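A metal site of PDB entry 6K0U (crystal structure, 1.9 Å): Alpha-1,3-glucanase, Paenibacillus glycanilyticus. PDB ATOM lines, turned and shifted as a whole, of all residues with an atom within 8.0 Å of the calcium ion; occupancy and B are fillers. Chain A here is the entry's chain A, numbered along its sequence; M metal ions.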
ATOM      1  N   ILE A  21      24.698  -0.975 -31.168  1.00  0.00           N
ATOM      2  CA  ILE A  21      23.972   0.001 -30.353  1.00  0.00           C
ATOM      3  C   ILE A  21      24.949   1.088 -29.955  1.00  0.00           C
ATOM      4  O   ILE A  21      26.034   0.783 -29.434  1.00  0.00           O
ATOM      5  CB  ILE A  21      23.342  -0.637 -29.103  1.00  0.00           C
ATOM      6  CG1 ILE A  21      22.385  -1.762 -29.459  1.00  0.00           C
ATOM      7  CG2 ILE A  21      22.649   0.448 -28.242  1.00  0.00           C
ATOM      8  CD1 ILE A  21      20.926  -1.326 -29.485  1.00  0.00           C
ATOM      9  N   MET A  22      24.567   2.343 -30.164  1.00  0.00           N
ATOM     10  CA  MET A  22      25.291   3.464 -29.579  1.00  0.00           C
ATOM     11  C   MET A  22      24.343   4.327 -28.766  1.00  0.00           C
ATOM     12  O   MET A  22      23.266   4.691 -29.256  1.00  0.00           O
ATOM     13  CB  MET A  22      25.930   4.345 -30.623  1.00  0.00           C
ATOM     14  CG  MET A  22      26.971   3.626 -31.390  1.00  0.00           C
ATOM     15  SD  MET A  22      26.829   4.222 -33.042  1.00  0.00           S
ATOM     16  CE  MET A  22      28.472   3.859 -33.597  1.00  0.00           C
ATOM     17  N   GLU A  23      24.763   4.666 -27.554  1.00  0.00           N
ATOM     18  CA  GLU A  23      24.007   5.597 -26.733  1.00  0.00           C
ATOM     19  C   GLU A  23      24.122   7.011 -27.298  1.00  0.00           C
ATOM     20  O   GLU A  23      25.211   7.455 -27.690  1.00  0.00           O
ATOM     21  CB  GLU A  23      24.529   5.551 -25.283  1.00  0.00           C
ATOM     22  CG  GLU A  23      24.350   4.173 -24.623  1.00  0.00           C
ATOM     23  CD  GLU A  23      22.881   3.809 -24.445  1.00  0.00           C
ATOM     24  OE1 GLU A  23      22.024   4.700 -24.543  1.00  0.00           O
ATOM     25  OE2 GLU A  23      22.580   2.625 -24.194  1.00  0.00           O
ATOM     26  N   ALA A  24      23.001   7.727 -27.342  1.00  0.00           N
ATOM     27  CA  ALA A  24      23.052   9.100 -27.830  1.00  0.00           C
ATOM     28  C   ALA A  24      24.015   9.945 -26.993  1.00  0.00           C
ATOM     29  O   ALA A  24      24.804  10.737 -27.530  1.00  0.00           O
ATOM     30  CB  ALA A  24      21.665   9.736 -27.826  1.00  0.00           C
ATOM     31  N   GLU A  25      23.992   9.754 -25.684  1.00  0.00           N
ATOM     32  CA  GLU A  25      24.778  10.506 -24.712  1.00  0.00           C
ATOM     33  C   GLU A  25      26.242  10.094 -24.667  1.00  0.00           C
ATOM     34  O   GLU A  25      27.000  10.660 -23.869  1.00  0.00           O
ATOM     35  CB  GLU A  25      24.151  10.336 -23.321  1.00  0.00           C
ATOM     36  CG  GLU A  25      24.242   8.940 -22.735  1.00  0.00           C
ATOM     37  CD  GLU A  25      23.082   8.024 -23.143  1.00  0.00           C
ATOM     38  OE1 GLU A  25      22.380   8.309 -24.143  1.00  0.00           O
ATOM     39  OE2 GLU A  25      22.872   7.009 -22.454  1.00  0.00           O
ATOM     40  N   SER A  26      26.673   9.138 -25.484  1.00  0.00           N
ATOM     41  CA  SER A  26      28.065   8.718 -25.486  1.00  0.00           C
ATOM     42  C   SER A  26      28.996   9.917 -25.620  1.00  0.00           C
ATOM     43  O   SER A  26      28.713  10.882 -26.332  1.00  0.00           O
ATOM     44  CB  SER A  26      28.325   7.725 -26.619  1.00  0.00           C
ATOM     45  OG  SER A  26      29.718   7.609 -26.832  1.00  0.00           O
ATOM     46  N   TYR A  45      12.462  10.734 -17.941  1.00  0.00           N
ATOM     47  CA  TYR A  45      13.105  10.529 -19.242  1.00  0.00           C
ATOM     48  C   TYR A  45      14.554  10.083 -19.110  1.00  0.00           C
ATOM     49  O   TYR A  45      15.087   9.462 -20.045  1.00  0.00           O
ATOM     50  CB  TYR A  45      13.003  11.809 -20.078  1.00  0.00           C
ATOM     51  CG  TYR A  45      11.586  12.054 -20.521  1.00  0.00           C
ATOM     52  CD1 TYR A  45      11.033  11.298 -21.554  1.00  0.00           C
ATOM     53  CD2 TYR A  45      10.787  12.989 -19.890  1.00  0.00           C
ATOM     54  CE1 TYR A  45       9.727  11.510 -21.955  1.00  0.00           C
ATOM     55  CE2 TYR A  45       9.474  13.201 -20.279  1.00  0.00           C
ATOM     56  CZ  TYR A  45       8.956  12.460 -21.310  1.00  0.00           C
ATOM     57  OH  TYR A  45       7.651  12.667 -21.695  1.00  0.00           O
ATOM     58  N   ALA A  46      15.195  10.340 -17.977  1.00  0.00           N
ATOM     59  CA  ALA A  46      16.521   9.755 -17.748  1.00  0.00           C
ATOM     60  C   ALA A  46      16.399   8.340 -17.195  1.00  0.00           C
ATOM     61  O   ALA A  46      16.997   7.391 -17.724  1.00  0.00           O
ATOM     62  CB  ALA A  46      17.339  10.655 -16.809  1.00  0.00           C
ATOM     63  N   GLU A  48      14.193   6.126 -17.437  1.00  0.00           N
ATOM     64  CA  GLU A  48      13.664   5.130 -18.355  1.00  0.00           C
ATOM     65  C   GLU A  48      14.525   4.969 -19.603  1.00  0.00           C
ATOM     66  O   GLU A  48      14.235   4.101 -20.430  1.00  0.00           O
ATOM     67  CB  GLU A  48      12.231   5.468 -18.755  1.00  0.00           C
ATOM     68  CG  GLU A  48      11.235   5.398 -17.603  1.00  0.00           C
ATOM     69  CD  GLU A  48       9.817   5.062 -18.053  1.00  0.00           C
ATOM     70  OE1 GLU A  48       9.595   4.804 -19.253  1.00  0.00           O
ATOM     71  OE2 GLU A  48       8.912   5.042 -17.196  1.00  0.00           O
ATOM     72  N   ALA A  49      15.571   5.762 -19.756  1.00  0.00           N
ATOM     73  CA  ALA A  49      16.450   5.668 -20.904  1.00  0.00           C
ATOM     74  C   ALA A  49      17.443   4.527 -20.752  1.00  0.00           C
ATOM     75  O   ALA A  49      17.838   4.169 -19.637  1.00  0.00           O
ATOM     76  CB  ALA A  49      17.215   6.981 -21.105  1.00  0.00           C
ATOM     77  N   SER A  50      17.855   3.957 -21.892  1.00  0.00           N
ATOM     78  CA  SER A  50      19.044   3.113 -21.913  1.00  0.00           C
ATOM     79  C   SER A  50      20.252   3.886 -21.398  1.00  0.00           C
ATOM     80  O   SER A  50      20.511   5.016 -21.809  1.00  0.00           O
ATOM     81  CB  SER A  50      19.302   2.614 -23.349  1.00  0.00           C
ATOM     82  OG  SER A  50      20.410   1.719 -23.398  1.00  0.00           O
ATOM     83  N   GLY A  51      20.989   3.260 -20.481  1.00  0.00           N
ATOM     84  CA  GLY A  51      22.121   3.921 -19.874  1.00  0.00           C
ATOM     85  C   GLY A  51      21.675   5.035 -18.961  1.00  0.00           C
ATOM     86  O   GLY A  51      22.491   5.855 -18.523  1.00  0.00           O
ATOM     87  N   ARG A  52      20.380   5.077 -18.652  1.00  0.00           N
ATOM     88  CA  ARG A  52      19.761   6.071 -17.772  1.00  0.00           C
ATOM     89  C   ARG A  52      20.041   7.499 -18.241  1.00  0.00           C
ATOM     90  O   ARG A  52      20.026   8.426 -17.421  1.00  0.00           O
ATOM     91  CB  ARG A  52      20.204   5.906 -16.312  1.00  0.00           C
ATOM     92  CG  ARG A  52      20.105   4.464 -15.812  1.00  0.00           C
ATOM     93  CD  ARG A  52      18.672   3.973 -15.788  1.00  0.00           C
ATOM     94  NE  ARG A  52      18.635   2.602 -15.300  1.00  0.00           N
ATOM     95  CZ  ARG A  52      17.654   2.066 -14.575  1.00  0.00           C
ATOM     96  NH1 ARG A  52      16.571   2.765 -14.232  1.00  0.00           N
ATOM     97  NH2 ARG A  52      17.771   0.808 -14.202  1.00  0.00           N
ATOM     98  N   SER A  53      20.284   7.703 -19.537  1.00  0.00           N
ATOM     99  CA  SER A  53      20.399   9.066 -20.039  1.00  0.00           C
ATOM    100  C   SER A  53      19.998   9.102 -21.514  1.00  0.00           C
ATOM    101  O   SER A  53      20.062   8.095 -22.223  1.00  0.00           O
ATOM    102  CB  SER A  53      21.819   9.611 -19.844  1.00  0.00           C
ATOM    103  OG  SER A  53      21.912  10.913 -20.377  1.00  0.00           O
ATOM    104  N   SER A  54      19.573  10.289 -21.948  1.00  0.00           N
ATOM    105  CA  SER A  54      19.322  10.535 -23.359  1.00  0.00           C
ATOM    106  C   SER A  54      19.707  11.978 -23.660  1.00  0.00           C
ATOM    107  O   SER A  54      20.082  12.741 -22.776  1.00  0.00           O
ATOM    108  CB  SER A  54      17.859  10.260 -23.719  1.00  0.00           C
ATOM    109  OG  SER A  54      17.008  11.025 -22.890  1.00  0.00           O
ATOM    110  N   VAL A  55      19.617  12.361 -24.941  1.00  0.00           N
ATOM    111  CA  VAL A  55      19.891  13.737 -25.335  1.00  0.00           C
ATOM    112  C   VAL A  55      18.587  14.379 -25.767  1.00  0.00           C
ATOM    113  O   VAL A  55      17.900  13.855 -26.654  1.00  0.00           O
ATOM    114  CB  VAL A  55      20.966  13.817 -26.429  1.00  0.00           C
ATOM    115  CG1 VAL A  55      21.250  15.279 -26.710  1.00  0.00           C
ATOM    116  CG2 VAL A  55      22.236  13.120 -25.945  1.00  0.00           C
ATOM    117  N   ARG A  78      15.729   4.815 -30.751  1.00  0.00           N
ATOM    118  CA  ARG A  78      14.913   4.812 -29.542  1.00  0.00           C
ATOM    119  C   ARG A  78      14.801   6.245 -29.049  1.00  0.00           C
ATOM    120  O   ARG A  78      15.810   6.946 -28.938  1.00  0.00           O
ATOM    121  CB  ARG A  78      15.489   3.893 -28.465  1.00  0.00           C
ATOM    122  CG  ARG A  78      14.478   3.571 -27.315  1.00  0.00           C
ATOM    123  CD  ARG A  78      15.087   2.697 -26.171  1.00  0.00           C
ATOM    124  NE  ARG A  78      14.065   2.054 -25.344  1.00  0.00           N
ATOM    125  CZ  ARG A  78      13.825   2.338 -24.060  1.00  0.00           C
ATOM    126  NH1 ARG A  78      14.546   3.251 -23.395  1.00  0.00           N
ATOM    127  NH2 ARG A  78      12.863   1.662 -23.418  1.00  0.00           N
ATOM    128  N   TYR A 136       9.587   5.620 -23.722  1.00  0.00           N
ATOM    129  CA  TYR A 136      10.379   5.515 -24.940  1.00  0.00           C
ATOM    130  C   TYR A 136       9.734   4.575 -25.941  1.00  0.00           C
ATOM    131  O   TYR A 136       8.955   3.693 -25.586  1.00  0.00           O
ATOM    132  CB  TYR A 136      11.821   5.072 -24.611  1.00  0.00           C
ATOM    133  CG  TYR A 136      12.621   6.207 -24.033  1.00  0.00           C
ATOM    134  CD1 TYR A 136      13.305   7.086 -24.862  1.00  0.00           C
ATOM    135  CD2 TYR A 136      12.644   6.458 -22.675  1.00  0.00           C
ATOM    136  CE1 TYR A 136      14.008   8.174 -24.353  1.00  0.00           C
ATOM    137  CE2 TYR A 136      13.349   7.541 -22.149  1.00  0.00           C
ATOM    138  CZ  TYR A 136      14.027   8.389 -23.006  1.00  0.00           C
ATOM    139  OH  TYR A 136      14.738   9.466 -22.525  1.00  0.00           O
ATOM    140  N   VAL A 167      16.462  11.702 -27.481  1.00  0.00           N
ATOM    141  CA  VAL A 167      17.182  10.720 -28.291  1.00  0.00           C
ATOM    142  C   VAL A 167      17.958   9.821 -27.332  1.00  0.00           C
ATOM    143  O   VAL A 167      18.866  10.279 -26.635  1.00  0.00           O
ATOM    144  CB  VAL A 167      18.129  11.410 -29.292  1.00  0.00           C
ATOM    145  CG1 VAL A 167      18.867  10.372 -30.135  1.00  0.00           C
ATOM    146  CG2 VAL A 167      17.334  12.379 -30.154  1.00  0.00           C
ATOM    147  N   ASP A 168      17.588   8.537 -27.297  1.00  0.00           N
ATOM    148  CA  ASP A 168      18.140   7.619 -26.297  1.00  0.00           C
ATOM    149  C   ASP A 168      19.318   6.827 -26.842  1.00  0.00           C
ATOM    150  O   ASP A 168      20.423   6.869 -26.288  1.00  0.00           O
ATOM    151  CB  ASP A 168      17.032   6.675 -25.799  1.00  0.00           C
ATOM    152  CG  ASP A 168      17.513   5.722 -24.701  1.00  0.00           C
ATOM    153  OD1 ASP A 168      18.631   5.904 -24.152  1.00  0.00           O
ATOM    154  OD2 ASP A 168      16.737   4.818 -24.330  1.00  0.00           O
ATOM    155  N   LEU A 169      19.099   6.067 -27.907  1.00  0.00           N
ATOM    156  CA  LEU A 169      20.149   5.260 -28.496  1.00  0.00           C
ATOM    157  C   LEU A 169      19.867   5.123 -29.986  1.00  0.00           C
ATOM    158  O   LEU A 169      18.773   5.445 -30.471  1.00  0.00           O
ATOM    159  CB  LEU A 169      20.284   3.882 -27.822  1.00  0.00           C
ATOM    160  CG  LEU A 169      19.092   2.884 -27.810  1.00  0.00           C
ATOM    161  CD1 LEU A 169      18.903   2.208 -29.160  1.00  0.00           C
ATOM    162  CD2 LEU A 169      19.261   1.786 -26.731  1.00  0.00           C
ATOM    163  N   LEU A 170      20.845   4.596 -30.698  1.00  0.00           N
ATOM    164  CA  LEU A 170      20.703   4.307 -32.121  1.00  0.00           C
ATOM    165  C   LEU A 170      21.211   2.900 -32.403  1.00  0.00           C
ATOM    166  O   LEU A 170      22.331   2.555 -32.049  1.00  0.00           O
ATOM    167  CB  LEU A 170      21.491   5.331 -32.953  1.00  0.00           C
ATOM    168  CG  LEU A 170      21.316   5.247 -34.465  1.00  0.00           C
ATOM    169  CD1 LEU A 170      19.940   5.771 -34.875  1.00  0.00           C
ATOM    170  CD2 LEU A 170      22.430   6.013 -35.167  1.00  0.00           C
ATOM    171  N   ASN A 382      16.347  -2.606 -20.911  1.00  0.00           N
ATOM    172  CA  ASN A 382      15.186  -1.715 -20.761  1.00  0.00           C
ATOM    173  C   ASN A 382      13.933  -2.487 -20.397  1.00  0.00           C
ATOM    174  O   ASN A 382      12.876  -2.344 -21.022  1.00  0.00           O
ATOM    175  CB  ASN A 382      14.941  -0.890 -22.027  1.00  0.00           C
ATOM    176  CG  ASN A 382      15.984   0.175 -22.219  1.00  0.00           C
ATOM    177  OD1 ASN A 382      16.684   0.198 -23.225  1.00  0.00           O
ATOM    178  ND2 ASN A 382      16.090   1.083 -21.256  1.00  0.00           N
ATOM    179  N   ASP A 406      19.344  -2.160 -17.103  1.00  0.00           N
ATOM    180  CA  ASP A 406      18.358  -1.072 -17.029  1.00  0.00           C
ATOM    181  C   ASP A 406      16.953  -1.607 -16.784  1.00  0.00           C
ATOM    182  O   ASP A 406      16.017  -1.390 -17.557  1.00  0.00           O
ATOM    183  CB  ASP A 406      18.429  -0.206 -18.286  1.00  0.00           C
ATOM    184  CG  ASP A 406      19.695   0.626 -18.321  1.00  0.00           C
ATOM    185  OD1 ASP A 406      20.070   1.142 -17.256  1.00  0.00           O
ATOM    186  OD2 ASP A 406      20.343   0.717 -19.392  1.00  0.00           O
ATOM    187  N   ARG A 441      23.214  -1.609 -14.030  1.00  0.00           N
ATOM    188  CA  ARG A 441      22.128  -0.767 -13.530  1.00  0.00           C
ATOM    189  C   ARG A 441      20.817  -1.550 -13.421  1.00  0.00           C
ATOM    190  O   ARG A 441      19.776  -1.137 -13.947  1.00  0.00           O
ATOM    191  CB  ARG A 441      21.987   0.472 -14.413  1.00  0.00           C
ATOM    192  CG  ARG A 441      23.311   1.243 -14.612  1.00  0.00           C
ATOM    193  CD  ARG A 441      23.183   2.369 -15.660  1.00  0.00           C
ATOM    194  NE  ARG A 441      22.805   1.807 -16.954  1.00  0.00           N
ATOM    195  CZ  ARG A 441      23.672   1.283 -17.797  1.00  0.00           C
ATOM    196  NH1 ARG A 441      24.957   1.287 -17.494  1.00  0.00           N
ATOM    197  NH2 ARG A 441      23.260   0.761 -18.947  1.00  0.00           N
HETATM  198 CA    CA M   1      20.828   6.448 -23.747  1.00  0.00          CA
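O of Asp 168 lies close to N of Ala 24 (2.9 Å). The side-chain carboxylate of Asp 168 lies within salt-bridge range of the guanidinium group of Arg 78, 2.9 Å away. The side-chain amide nitrogen (ND2) of Asn 382 lies close to the backbone NH (N) of Ser 50, at 3.4 Å.
Within 4 Å of the calcium ion: Glu 23, Glu 25, Ser 50, Ser 53 and Asp 168. The nearest printed residue that does not touch the calcium ion is Ser 54 (4.4 Å).
The calcium ion is bound by OE1 of Glu 23 (2.3 Å), OD1 of Asp 168 (2.3 Å), O of Ser 53 (2.4 Å), O of Ser 50 (2.4 Å), OE1 of Glu 25 (2.5 Å), OE2 of Glu 25 (2.5 Å) and O of Asp 168 (2.6 Å).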
